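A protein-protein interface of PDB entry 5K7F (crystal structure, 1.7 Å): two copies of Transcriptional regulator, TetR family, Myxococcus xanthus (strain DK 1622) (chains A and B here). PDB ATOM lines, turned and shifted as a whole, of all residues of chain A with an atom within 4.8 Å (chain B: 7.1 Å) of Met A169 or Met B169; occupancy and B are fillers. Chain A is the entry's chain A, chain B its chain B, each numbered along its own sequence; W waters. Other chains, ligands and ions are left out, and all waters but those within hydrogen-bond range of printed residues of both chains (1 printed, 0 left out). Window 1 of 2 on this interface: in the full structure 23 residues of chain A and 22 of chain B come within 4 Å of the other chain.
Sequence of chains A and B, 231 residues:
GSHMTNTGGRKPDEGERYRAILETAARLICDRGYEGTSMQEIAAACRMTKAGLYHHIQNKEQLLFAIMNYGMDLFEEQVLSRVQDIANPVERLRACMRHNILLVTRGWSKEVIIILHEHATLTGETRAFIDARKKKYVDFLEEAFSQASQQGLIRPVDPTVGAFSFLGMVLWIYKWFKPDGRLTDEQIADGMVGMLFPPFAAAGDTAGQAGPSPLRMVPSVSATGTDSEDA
Of the printed residues of chain B, Ser A165 touches Met B169, Met B192 and Met B195.
Of chain B, only Gly B168 and Trp B172 come within 4 Å of Gly A168.
Printed residues of chain B within 4 Å of Met A169: Ser B165, Gly B168 and Met B169.
Of chain A, only Ser A165 and Met A169 come within 4 Å of Met B169.
Val B170 touches none of the printed residues of chain A.
Ile B173 touches none of the printed residues of chain A.
Of the printed residues of chain A, Met B192 touches Ser A165.
Of the 22 printed residues of chain B, 9 touch a printed residue of chain A.
Hydrophobic or aromatic side chains of chain B that line the printed part of chain A: Val B161, Phe B164, Met B169, Leu B171, Trp B172, Met B192 and Met B195.
Among the printed residues, no Asp or Glu carboxylate lies within 4 Å of a Lys or Arg side-chain nitrogen of the other chain.
Ser A165 touches Met B192, and with the chains exchanged Met A192 touches Ser B165.
Gly B168 touches its own counterpart, Gly A168.
Gly A168 touches Trp B172, and with the chains exchanged Trp A172 touches Gly B168.
Leu A171 touches Trp B172, and with the chains exchanged Trp A172 touches Leu B171.
Positions printed for both chains: 97, 165, 166, 167, 168, 169, 170, 171, 172, 173, 192 and 196.
The backbone carbonyl oxygen (O) of Val B161 sits at hydrogen-bond distance from the side-chain hydroxyl (OG) of Ser B165 (2.7 Å).
O of Gly A168 sits close to O of Gly B168, 3.4 Å away.
Water W1 lies within hydrogen-bond range of O of Phe B164 and O of Met A169.
Among the printed residues, pairs that only touch across the chains: Leu A171 with Trp B172 (3.3 Å), Met A169 with Met B169 (3.4 Å), Met A169 with Ser B165 (3.5 Å), Gly A168 with Trp B172 (3.5 Å), Ser A165 with Met B169 (3.5 Å), Trp A172 with Leu B171 (3.5 Å), Met A192 with Ser B165 (3.6 Å), Trp A172 with Gly B168 (3.6 Å), Ser A165 with Met B192 (3.7 Å), Leu A196 with Met B195 (3.8 Å), Trp A172 with Phe B164 (3.8 Å), Ser A165 with Met B195 (3.8 Å), Met A192 with Val B161 (3.8 Å), Met A169 with Gly B168 (3.9 Å) and Trp A172 with Trp B172 (3.9 Å).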
ATOM      1  N   MET A  97      -0.158 -15.175  -7.748  1.00  0.00           N
ATOM      2  CA  MET A  97       1.252 -14.963  -7.474  1.00  0.00           C
ATOM      3  C   MET A  97       2.133 -15.819  -8.376  1.00  0.00           C
ATOM      4  O   MET A  97       3.135 -15.332  -8.923  1.00  0.00           O
ATOM      5  CB  MET A  97       1.568 -15.282  -6.020  1.00  0.00           C
ATOM      6  CG  MET A  97       3.030 -14.970  -5.692  1.00  0.00           C
ATOM      7  SD  MET A  97       3.384 -15.104  -3.932  1.00  0.00           S
ATOM      8  CE  MET A  97       3.599 -13.391  -3.538  1.00  0.00           C
ATOM      9  N   SER A 165       2.552  -5.667  -0.815  1.00  0.00           N
ATOM     10  CA  SER A 165       3.609  -6.600  -0.404  1.00  0.00           C
ATOM     11  C   SER A 165       3.810  -7.643  -1.492  1.00  0.00           C
ATOM     12  O   SER A 165       4.946  -7.912  -1.953  1.00  0.00           O
ATOM     13  CB  SER A 165       3.244  -7.264   0.923  1.00  0.00           C
ATOM     14  OG  SER A 165       3.240  -6.296   1.981  1.00  0.00           O
ATOM     15  N   PHE A 166       2.697  -8.218  -1.916  1.00  0.00           N
ATOM     16  CA  PHE A 166       2.627  -9.123  -3.061  1.00  0.00           C
ATOM     17  C   PHE A 166       3.301  -8.507  -4.286  1.00  0.00           C
ATOM     18  O   PHE A 166       4.149  -9.138  -4.947  1.00  0.00           O
ATOM     19  CB  PHE A 166       1.147  -9.408  -3.289  1.00  0.00           C
ATOM     20  CG  PHE A 166       0.807 -10.282  -4.494  1.00  0.00           C
ATOM     21  CD1 PHE A 166       1.114  -9.921  -5.804  1.00  0.00           C
ATOM     22  CD2 PHE A 166       0.049 -11.392  -4.280  1.00  0.00           C
ATOM     23  CE1 PHE A 166       0.699 -10.753  -6.896  1.00  0.00           C
ATOM     24  CE2 PHE A 166      -0.363 -12.197  -5.342  1.00  0.00           C
ATOM     25  CZ  PHE A 166      -0.023 -11.837  -6.648  1.00  0.00           C
ATOM     26  N   LEU A 167       2.885  -7.292  -4.655  1.00  0.00           N
ATOM     27  CA  LEU A 167       3.435  -6.661  -5.844  1.00  0.00           C
ATOM     28  C   LEU A 167       4.937  -6.410  -5.720  1.00  0.00           C
ATOM     29  O   LEU A 167       5.692  -6.678  -6.663  1.00  0.00           O
ATOM     30  CB  LEU A 167       2.695  -5.358  -6.135  1.00  0.00           C
ATOM     31  CG  LEU A 167       1.380  -5.495  -6.880  1.00  0.00           C
ATOM     32  CD1 LEU A 167       0.699  -4.114  -6.951  1.00  0.00           C
ATOM     33  CD2 LEU A 167       1.581  -6.101  -8.281  1.00  0.00           C
ATOM     34  N   GLY A 168       5.403  -5.858  -4.587  1.00  0.00           N
ATOM     35  CA  GLY A 168       6.835  -5.641  -4.433  1.00  0.00           C
ATOM     36  C   GLY A 168       7.625  -6.940  -4.512  1.00  0.00           C
ATOM     37  O   GLY A 168       8.675  -7.005  -5.154  1.00  0.00           O
ATOM     38  N   MET A 169       7.199  -7.950  -3.764  1.00  0.00           N
ATOM     39  CA  MET A 169       7.885  -9.246  -3.849  1.00  0.00           C
ATOM     40  C   MET A 169       8.048  -9.699  -5.283  1.00  0.00           C
ATOM     41  O   MET A 169       9.144 -10.136  -5.687  1.00  0.00           O
ATOM     42  CB  MET A 169       7.121 -10.327  -3.076  1.00  0.00           C
ATOM     43  CG  MET A 169       7.303 -10.313  -1.620  1.00  0.00           C
ATOM     44  SD  MET A 169       6.164 -11.474  -0.808  1.00  0.00           S
ATOM     45  CE  MET A 169       6.655 -12.992  -1.521  1.00  0.00           C
ATOM     46  N   VAL A 170       6.990  -9.583  -6.075  1.00  0.00           N
ATOM     47  CA  VAL A 170       6.980 -10.247  -7.384  1.00  0.00           C
ATOM     48  C   VAL A 170       7.668  -9.387  -8.428  1.00  0.00           C
ATOM     49  O   VAL A 170       8.502  -9.877  -9.198  1.00  0.00           O
ATOM     50  CB  VAL A 170       5.537 -10.586  -7.785  1.00  0.00           C
ATOM     51  CG1 VAL A 170       5.501 -11.161  -9.169  1.00  0.00           C
ATOM     52  CG2 VAL A 170       4.965 -11.599  -6.781  1.00  0.00           C
ATOM     53  N   LEU A 171       7.387  -8.083  -8.450  1.00  0.00           N
ATOM     54  CA  LEU A 171       7.939  -7.265  -9.515  1.00  0.00           C
ATOM     55  C   LEU A 171       9.442  -7.068  -9.348  1.00  0.00           C
ATOM     56  O   LEU A 171      10.152  -6.882 -10.346  1.00  0.00           O
ATOM     57  CB  LEU A 171       7.203  -5.918  -9.566  1.00  0.00           C
ATOM     58  CG  LEU A 171       5.705  -6.037  -9.861  1.00  0.00           C
ATOM     59  CD1 LEU A 171       5.076  -4.651  -9.847  1.00  0.00           C
ATOM     60  CD2 LEU A 171       5.462  -6.718 -11.188  1.00  0.00           C
ATOM     61  N   TRP A 172       9.955  -7.082  -8.107  1.00  0.00           N
ATOM     62  CA  TRP A 172      11.382  -6.875  -7.871  1.00  0.00           C
ATOM     63  C   TRP A 172      12.233  -8.074  -8.293  1.00  0.00           C
ATOM     64  O   TRP A 172      13.463  -7.934  -8.352  1.00  0.00           O
ATOM     65  CB  TRP A 172      11.640  -6.505  -6.391  1.00  0.00           C
ATOM     66  CG  TRP A 172      12.836  -5.544  -6.242  1.00  0.00           C
ATOM     67  CD1 TRP A 172      12.882  -4.232  -6.629  1.00  0.00           C
ATOM     68  CD2 TRP A 172      14.138  -5.848  -5.723  1.00  0.00           C
ATOM     69  NE1 TRP A 172      14.120  -3.708  -6.380  1.00  0.00           N
ATOM     70  CE2 TRP A 172      14.908  -4.673  -5.818  1.00  0.00           C
ATOM     71  CE3 TRP A 172      14.727  -6.992  -5.178  1.00  0.00           C
ATOM     72  CZ2 TRP A 172      16.233  -4.610  -5.385  1.00  0.00           C
ATOM     73  CZ3 TRP A 172      16.062  -6.922  -4.755  1.00  0.00           C
ATOM     74  CH2 TRP A 172      16.786  -5.751  -4.874  1.00  0.00           C
ATOM     75  N   ILE A 173      11.615  -9.224  -8.634  1.00  0.00           N
ATOM     76  CA  ILE A 173      12.354 -10.419  -9.086  1.00  0.00           C
ATOM     77  C   ILE A 173      13.266 -10.111 -10.278  1.00  0.00           C
ATOM     78  O   ILE A 173      14.339 -10.705 -10.411  1.00  0.00           O
ATOM     79  CB  ILE A 173      11.384 -11.554  -9.397  1.00  0.00           C
ATOM     80  CG1 ILE A 173      10.631 -12.000  -8.132  1.00  0.00           C
ATOM     81  CG2 ILE A 173      12.128 -12.724 -10.008  1.00  0.00           C
ATOM     82  CD1 ILE A 173       9.545 -13.140  -8.422  1.00  0.00           C
ATOM     83  N   MET A 192       7.801 -18.274  -2.391  1.00  0.00           N
ATOM     84  CA  MET A 192       7.100 -17.015  -2.117  1.00  0.00           C
ATOM     85  C   MET A 192       5.658 -17.276  -1.704  1.00  0.00           C
ATOM     86  O   MET A 192       5.142 -16.664  -0.760  1.00  0.00           O
ATOM     87  CB  MET A 192       7.145 -16.110  -3.341  1.00  0.00           C
ATOM     88  CG  MET A 192       8.480 -15.376  -3.487  1.00  0.00           C
ATOM     89  SD  MET A 192       8.464 -14.028  -4.696  1.00  0.00           S
ATOM     90  CE  MET A 192      10.204 -13.719  -4.743  1.00  0.00           C
ATOM     91  N   LEU A 196       3.756 -16.158   1.956  1.00  0.00           N
ATOM     92  CA  LEU A 196       2.620 -15.267   2.127  1.00  0.00           C
ATOM     93  C   LEU A 196       1.325 -16.011   2.360  1.00  0.00           C
ATOM     94  O   LEU A 196       0.456 -15.514   3.093  1.00  0.00           O
ATOM     95  CB  LEU A 196       2.466 -14.367   0.902  1.00  0.00           C
ATOM     96  CG  LEU A 196       3.202 -13.029   0.858  1.00  0.00           C
ATOM     97  CD1 LEU A 196       2.413 -12.043   0.012  1.00  0.00           C
ATOM     98  CD2 LEU A 196       3.508 -12.416   2.233  1.00  0.00           C
ATOM     99  N   MET B  97      13.618  -5.007   9.124  1.00  0.00           N
ATOM    100  CA  MET B  97      12.573  -4.669   8.170  1.00  0.00           C
ATOM    101  C   MET B  97      11.886  -3.377   8.552  1.00  0.00           C
ATOM    102  O   MET B  97      11.638  -2.530   7.688  1.00  0.00           O
ATOM    103  CB  MET B  97      11.564  -5.818   8.049  1.00  0.00           C
ATOM    104  CG  MET B  97      10.532  -5.517   6.981  1.00  0.00           C
ATOM    105  SD  MET B  97       9.337  -6.805   6.691  1.00  0.00           S
ATOM    106  CE  MET B  97       9.485  -6.862   4.918  1.00  0.00           C
ATOM    107  N   ILE B 101      11.918   0.059   6.292  1.00  0.00           N
ATOM    108  CA  ILE B 101      10.678   0.675   5.819  1.00  0.00           C
ATOM    109  C   ILE B 101      10.679   2.131   6.214  1.00  0.00           C
ATOM    110  O   ILE B 101      10.356   3.024   5.421  1.00  0.00           O
ATOM    111  CB  ILE B 101       9.440  -0.037   6.399  1.00  0.00           C
ATOM    112  CG1 ILE B 101       9.265  -1.465   5.749  1.00  0.00           C
ATOM    113  CG2 ILE B 101       8.179   0.823   6.175  1.00  0.00           C
ATOM    114  CD1 ILE B 101       8.301  -2.338   6.442  1.00  0.00           C
ATOM    115  N   VAL B 161      15.154 -16.854  -1.014  1.00  0.00           N
ATOM    116  CA  VAL B 161      13.749 -16.497  -1.220  1.00  0.00           C
ATOM    117  C   VAL B 161      13.284 -15.541  -0.137  1.00  0.00           C
ATOM    118  O   VAL B 161      12.555 -14.573  -0.403  1.00  0.00           O
ATOM    119  CB  VAL B 161      12.867 -17.752  -1.260  1.00  0.00           C
ATOM    120  CG1 VAL B 161      11.379 -17.386  -1.318  1.00  0.00           C
ATOM    121  CG2 VAL B 161      13.254 -18.569  -2.470  1.00  0.00           C
ATOM    122  N   ALA B 163      15.180 -13.434   1.882  1.00  0.00           N
ATOM    123  CA  ALA B 163      15.886 -12.177   1.707  1.00  0.00           C
ATOM    124  C   ALA B 163      15.291 -11.339   0.578  1.00  0.00           C
ATOM    125  O   ALA B 163      15.139 -10.116   0.695  1.00  0.00           O
ATOM    126  CB  ALA B 163      17.365 -12.476   1.431  1.00  0.00           C
ATOM    127  N   PHE B 164      15.070 -11.959  -0.569  1.00  0.00           N
ATOM    128  CA  PHE B 164      14.601 -11.167  -1.699  1.00  0.00           C
ATOM    129  C   PHE B 164      13.121 -10.880  -1.651  1.00  0.00           C
ATOM    130  O   PHE B 164      12.671  -9.944  -2.336  1.00  0.00           O
ATOM    131  CB  PHE B 164      14.993 -11.857  -2.996  1.00  0.00           C
ATOM    132  CG  PHE B 164      16.460 -11.696  -3.297  1.00  0.00           C
ATOM    133  CD1 PHE B 164      17.007 -10.413  -3.478  1.00  0.00           C
ATOM    134  CD2 PHE B 164      17.306 -12.774  -3.333  1.00  0.00           C
ATOM    135  CE1 PHE B 164      18.356 -10.237  -3.732  1.00  0.00           C
ATOM    136  CE2 PHE B 164      18.658 -12.607  -3.597  1.00  0.00           C
ATOM    137  CZ  PHE B 164      19.187 -11.340  -3.785  1.00  0.00           C
ATOM    138  N   SER B 165      12.345 -11.637  -0.887  1.00  0.00           N
ATOM    139  CA  SER B 165      10.950 -11.249  -0.655  1.00  0.00           C
ATOM    140  C   SER B 165      10.917 -10.030   0.252  1.00  0.00           C
ATOM    141  O   SER B 165      10.145  -9.083   0.033  1.00  0.00           O
ATOM    142  CB  SER B 165      10.189 -12.383   0.002  1.00  0.00           C
ATOM    143  OG  SER B 165      10.049 -13.537  -0.860  1.00  0.00           O
ATOM    144  N   PHE B 166      11.710 -10.101   1.305  1.00  0.00           N
ATOM    145  CA  PHE B 166      11.927  -8.952   2.201  1.00  0.00           C
ATOM    146  C   PHE B 166      12.316  -7.709   1.396  1.00  0.00           C
ATOM    147  O   PHE B 166      11.655  -6.661   1.465  1.00  0.00           O
ATOM    148  CB  PHE B 166      12.981  -9.385   3.230  1.00  0.00           C
ATOM    149  CG  PHE B 166      13.498  -8.313   4.171  1.00  0.00           C
ATOM    150  CD1 PHE B 166      14.102  -7.150   3.742  1.00  0.00           C
ATOM    151  CD2 PHE B 166      13.485  -8.587   5.534  1.00  0.00           C
ATOM    152  CE1 PHE B 166      14.619  -6.255   4.674  1.00  0.00           C
ATOM    153  CE2 PHE B 166      14.014  -7.680   6.453  1.00  0.00           C
ATOM    154  CZ  PHE B 166      14.584  -6.552   6.021  1.00  0.00           C
ATOM    155  N   LEU B 167      13.388  -7.805   0.600  1.00  0.00           N
ATOM    156  CA  LEU B 167      13.887  -6.643  -0.126  1.00  0.00           C
ATOM    157  C   LEU B 167      12.862  -6.147  -1.146  1.00  0.00           C
ATOM    158  O   LEU B 167      12.658  -4.945  -1.278  1.00  0.00           O
ATOM    159  CB  LEU B 167      15.224  -6.949  -0.797  1.00  0.00           C
ATOM    160  CG  LEU B 167      16.398  -7.067   0.166  1.00  0.00           C
ATOM    161  CD1 LEU B 167      17.545  -7.670  -0.635  1.00  0.00           C
ATOM    162  CD2 LEU B 167      16.764  -5.729   0.721  1.00  0.00           C
ATOM    163  N   GLY B 168      12.189  -7.046  -1.868  1.00  0.00           N
ATOM    164  CA  GLY B 168      11.168  -6.577  -2.801  1.00  0.00           C
ATOM    165  C   GLY B 168      10.008  -5.868  -2.129  1.00  0.00           C
ATOM    166  O   GLY B 168       9.525  -4.859  -2.639  1.00  0.00           O
ATOM    167  N   MET B 169       9.576  -6.345  -0.960  1.00  0.00           N
ATOM    168  CA  MET B 169       8.474  -5.669  -0.300  1.00  0.00           C
ATOM    169  C   MET B 169       8.896  -4.261   0.103  1.00  0.00           C
ATOM    170  O   MET B 169       8.148  -3.311  -0.123  1.00  0.00           O
ATOM    171  CB  MET B 169       7.998  -6.465   0.935  1.00  0.00           C
ATOM    172  CG  MET B 169       7.328  -7.840   0.662  1.00  0.00           C
ATOM    173  SD  MET B 169       7.048  -8.730   2.220  1.00  0.00           S
ATOM    174  CE  MET B 169       6.279  -7.541   3.271  1.00  0.00           C
ATOM    175  N   VAL B 170      10.097  -4.111   0.662  1.00  0.00           N
ATOM    176  CA  VAL B 170      10.518  -2.801   1.192  1.00  0.00           C
ATOM    177  C   VAL B 170      10.921  -1.863   0.063  1.00  0.00           C
ATOM    178  O   VAL B 170      10.550  -0.682   0.065  1.00  0.00           O
ATOM    179  CB  VAL B 170      11.648  -2.972   2.224  1.00  0.00           C
ATOM    180  CG1 VAL B 170      12.066  -1.566   2.810  1.00  0.00           C
ATOM    181  CG2 VAL B 170      11.206  -3.869   3.329  1.00  0.00           C
ATOM    182  N   LEU B 171      11.686  -2.362  -0.932  1.00  0.00           N
ATOM    183  CA  LEU B 171      12.271  -1.463  -1.918  1.00  0.00           C
ATOM    184  C   LEU B 171      11.272  -0.985  -2.959  1.00  0.00           C
ATOM    185  O   LEU B 171      11.562  -0.008  -3.666  1.00  0.00           O
ATOM    186  CB  LEU B 171      13.459  -2.141  -2.594  1.00  0.00           C
ATOM    187  CG  LEU B 171      14.544  -2.416  -1.546  1.00  0.00           C
ATOM    188  CD1 LEU B 171      15.763  -3.018  -2.249  1.00  0.00           C
ATOM    189  CD2 LEU B 171      14.996  -1.198  -0.681  1.00  0.00           C
ATOM    190  N   TRP B 172      10.116  -1.657  -3.076  1.00  0.00           N
ATOM    191  CA  TRP B 172       9.038  -1.201  -3.950  1.00  0.00           C
ATOM    192  C   TRP B 172       8.242  -0.028  -3.350  1.00  0.00           C
ATOM    193  O   TRP B 172       7.521   0.656  -4.094  1.00  0.00           O
ATOM    194  CB  TRP B 172       8.105  -2.376  -4.236  1.00  0.00           C
ATOM    195  CG  TRP B 172       7.409  -2.274  -5.564  1.00  0.00           C
ATOM    196  CD1 TRP B 172       6.092  -1.978  -5.786  1.00  0.00           C
ATOM    197  CD2 TRP B 172       8.007  -2.430  -6.841  1.00  0.00           C
ATOM    198  NE1 TRP B 172       5.838  -1.941  -7.138  1.00  0.00           N
ATOM    199  CE2 TRP B 172       7.002  -2.201  -7.808  1.00  0.00           C
ATOM    200  CE3 TRP B 172       9.300  -2.700  -7.262  1.00  0.00           C
ATOM    201  CZ2 TRP B 172       7.254  -2.268  -9.164  1.00  0.00           C
ATOM    202  CZ3 TRP B 172       9.547  -2.775  -8.612  1.00  0.00           C
ATOM    203  CH2 TRP B 172       8.525  -2.565  -9.549  1.00  0.00           C
ATOM    204  N   ILE B 173       8.295   0.161  -2.021  1.00  0.00           N
ATOM    205  CA  ILE B 173       7.420   1.133  -1.353  1.00  0.00           C
ATOM    206  C   ILE B 173       7.426   2.459  -2.085  1.00  0.00           C
ATOM    207  O   ILE B 173       6.357   3.025  -2.353  1.00  0.00           O
ATOM    208  CB  ILE B 173       7.803   1.277   0.134  1.00  0.00           C
ATOM    209  CG1 ILE B 173       7.355   0.003   0.845  1.00  0.00           C
ATOM    210  CG2 ILE B 173       7.136   2.499   0.741  1.00  0.00           C
ATOM    211  CD1 ILE B 173       7.777  -0.148   2.321  1.00  0.00           C
ATOM    212  N   TYR B 174       8.617   2.954  -2.487  1.00  0.00           N
ATOM    213  CA  TYR B 174       8.690   4.336  -2.989  1.00  0.00           C
ATOM    214  C   TYR B 174       7.877   4.511  -4.270  1.00  0.00           C
ATOM    215  O   TYR B 174       7.488   5.634  -4.614  1.00  0.00           O
ATOM    216  CB  TYR B 174      10.136   4.744  -3.210  1.00  0.00           C
ATOM    217  CG  TYR B 174      10.716   4.395  -4.530  1.00  0.00           C
ATOM    218  CD1 TYR B 174      11.305   3.166  -4.742  1.00  0.00           C
ATOM    219  CD2 TYR B 174      10.709   5.305  -5.568  1.00  0.00           C
ATOM    220  CE1 TYR B 174      11.853   2.847  -5.950  1.00  0.00           C
ATOM    221  CE2 TYR B 174      11.263   4.990  -6.784  1.00  0.00           C
ATOM    222  CZ  TYR B 174      11.830   3.757  -6.967  1.00  0.00           C
ATOM    223  OH  TYR B 174      12.381   3.438  -8.181  1.00  0.00           O
ATOM    224  N   TRP B 176       4.770   3.415  -4.800  1.00  0.00           N
ATOM    225  CA  TRP B 176       3.324   3.457  -4.595  1.00  0.00           C
ATOM    226  C   TRP B 176       2.902   4.319  -3.406  1.00  0.00           C
ATOM    227  O   TRP B 176       1.801   4.886  -3.397  1.00  0.00           O
ATOM    228  CB  TRP B 176       2.761   2.054  -4.409  1.00  0.00           C
ATOM    229  CG  TRP B 176       3.275   1.218  -3.285  1.00  0.00           C
ATOM    230  CD1 TRP B 176       4.317   0.308  -3.334  1.00  0.00           C
ATOM    231  CD2 TRP B 176       2.717   1.104  -1.976  1.00  0.00           C
ATOM    232  NE1 TRP B 176       4.430  -0.343  -2.137  1.00  0.00           N
ATOM    233  CE2 TRP B 176       3.483   0.145  -1.279  1.00  0.00           C
ATOM    234  CE3 TRP B 176       1.674   1.743  -1.310  1.00  0.00           C
ATOM    235  CZ2 TRP B 176       3.236  -0.186   0.043  1.00  0.00           C
ATOM    236  CZ3 TRP B 176       1.432   1.404   0.006  1.00  0.00           C
ATOM    237  CH2 TRP B 176       2.223   0.454   0.675  1.00  0.00           C
ATOM    238  N   ILE B 188       2.003   0.543   7.564  1.00  0.00           N
ATOM    239  CA  ILE B 188       2.664  -0.278   6.553  1.00  0.00           C
ATOM    240  C   ILE B 188       3.759  -1.127   7.188  1.00  0.00           C
ATOM    241  O   ILE B 188       3.906  -2.326   6.892  1.00  0.00           O
ATOM    242  CB  ILE B 188       3.227   0.627   5.447  1.00  0.00           C
ATOM    243  CG1 ILE B 188       2.063   1.312   4.712  1.00  0.00           C
ATOM    244  CG2 ILE B 188       4.121  -0.181   4.474  1.00  0.00           C
ATOM    245  CD1 ILE B 188       2.490   2.349   3.712  1.00  0.00           C
ATOM    246  N   GLY B 191       2.153  -3.864   9.264  1.00  0.00           N
ATOM    247  CA  GLY B 191       1.501  -4.901   8.460  1.00  0.00           C
ATOM    248  C   GLY B 191       2.495  -5.805   7.758  1.00  0.00           C
ATOM    249  O   GLY B 191       2.415  -7.018   7.874  1.00  0.00           O
ATOM    250  N   MET B 192       3.459  -5.208   7.062  1.00  0.00           N
ATOM    251  CA  MET B 192       4.548  -5.936   6.419  1.00  0.00           C
ATOM    252  C   MET B 192       5.302  -6.865   7.369  1.00  0.00           C
ATOM    253  O   MET B 192       5.494  -8.059   7.060  1.00  0.00           O
ATOM    254  CB  MET B 192       5.517  -4.960   5.755  1.00  0.00           C
ATOM    255  CG  MET B 192       4.961  -4.242   4.488  1.00  0.00           C
ATOM    256  SD  MET B 192       6.220  -3.592   3.394  1.00  0.00           S
ATOM    257  CE  MET B 192       5.225  -2.970   2.048  1.00  0.00           C
ATOM    258  N   VAL B 193       5.797  -6.339   8.493  1.00  0.00           N
ATOM    259  CA  VAL B 193       6.504  -7.183   9.448  1.00  0.00           C
ATOM    260  C   VAL B 193       5.618  -8.323   9.912  1.00  0.00           C
ATOM    261  O   VAL B 193       6.074  -9.467  10.044  1.00  0.00           O
ATOM    262  CB  VAL B 193       7.004  -6.344  10.640  1.00  0.00           C
ATOM    263  CG1 VAL B 193       7.581  -7.261  11.721  1.00  0.00           C
ATOM    264  CG2 VAL B 193       8.034  -5.346  10.179  1.00  0.00           C
ATOM    265  N   MET B 195       3.318  -9.751   8.321  1.00  0.00           N
ATOM    266  CA  MET B 195       3.080 -10.708   7.244  1.00  0.00           C
ATOM    267  C   MET B 195       4.209 -11.716   7.144  1.00  0.00           C
ATOM    268  O   MET B 195       3.957 -12.919   6.982  1.00  0.00           O
ATOM    269  CB  MET B 195       2.952 -10.000   5.898  1.00  0.00           C
ATOM    270  CG  MET B 195       1.613  -9.448   5.612  1.00  0.00           C
ATOM    271  SD  MET B 195       1.473  -9.146   3.850  1.00  0.00           S
ATOM    272  CE  MET B 195       0.472 -10.514   3.532  1.00  0.00           C
ATOM    273  N   LEU B 196       5.460 -11.239   7.128  1.00  0.00           N
ATOM    274  CA  LEU B 196       6.592 -12.146   6.957  1.00  0.00           C
ATOM    275  C   LEU B 196       7.012 -12.800   8.259  1.00  0.00           C
ATOM    276  O   LEU B 196       7.561 -13.904   8.245  1.00  0.00           O
ATOM    277  CB  LEU B 196       7.817 -11.419   6.391  1.00  0.00           C
ATOM    278  CG  LEU B 196       7.893 -11.015   4.941  1.00  0.00           C
ATOM    279  CD1 LEU B 196       9.334 -10.697   4.645  1.00  0.00           C
ATOM    280  CD2 LEU B 196       7.392 -12.154   4.025  1.00  0.00           C
HETATM  281  O   HOH W   1      11.915 -10.151  -5.010  1.00  0.00           O
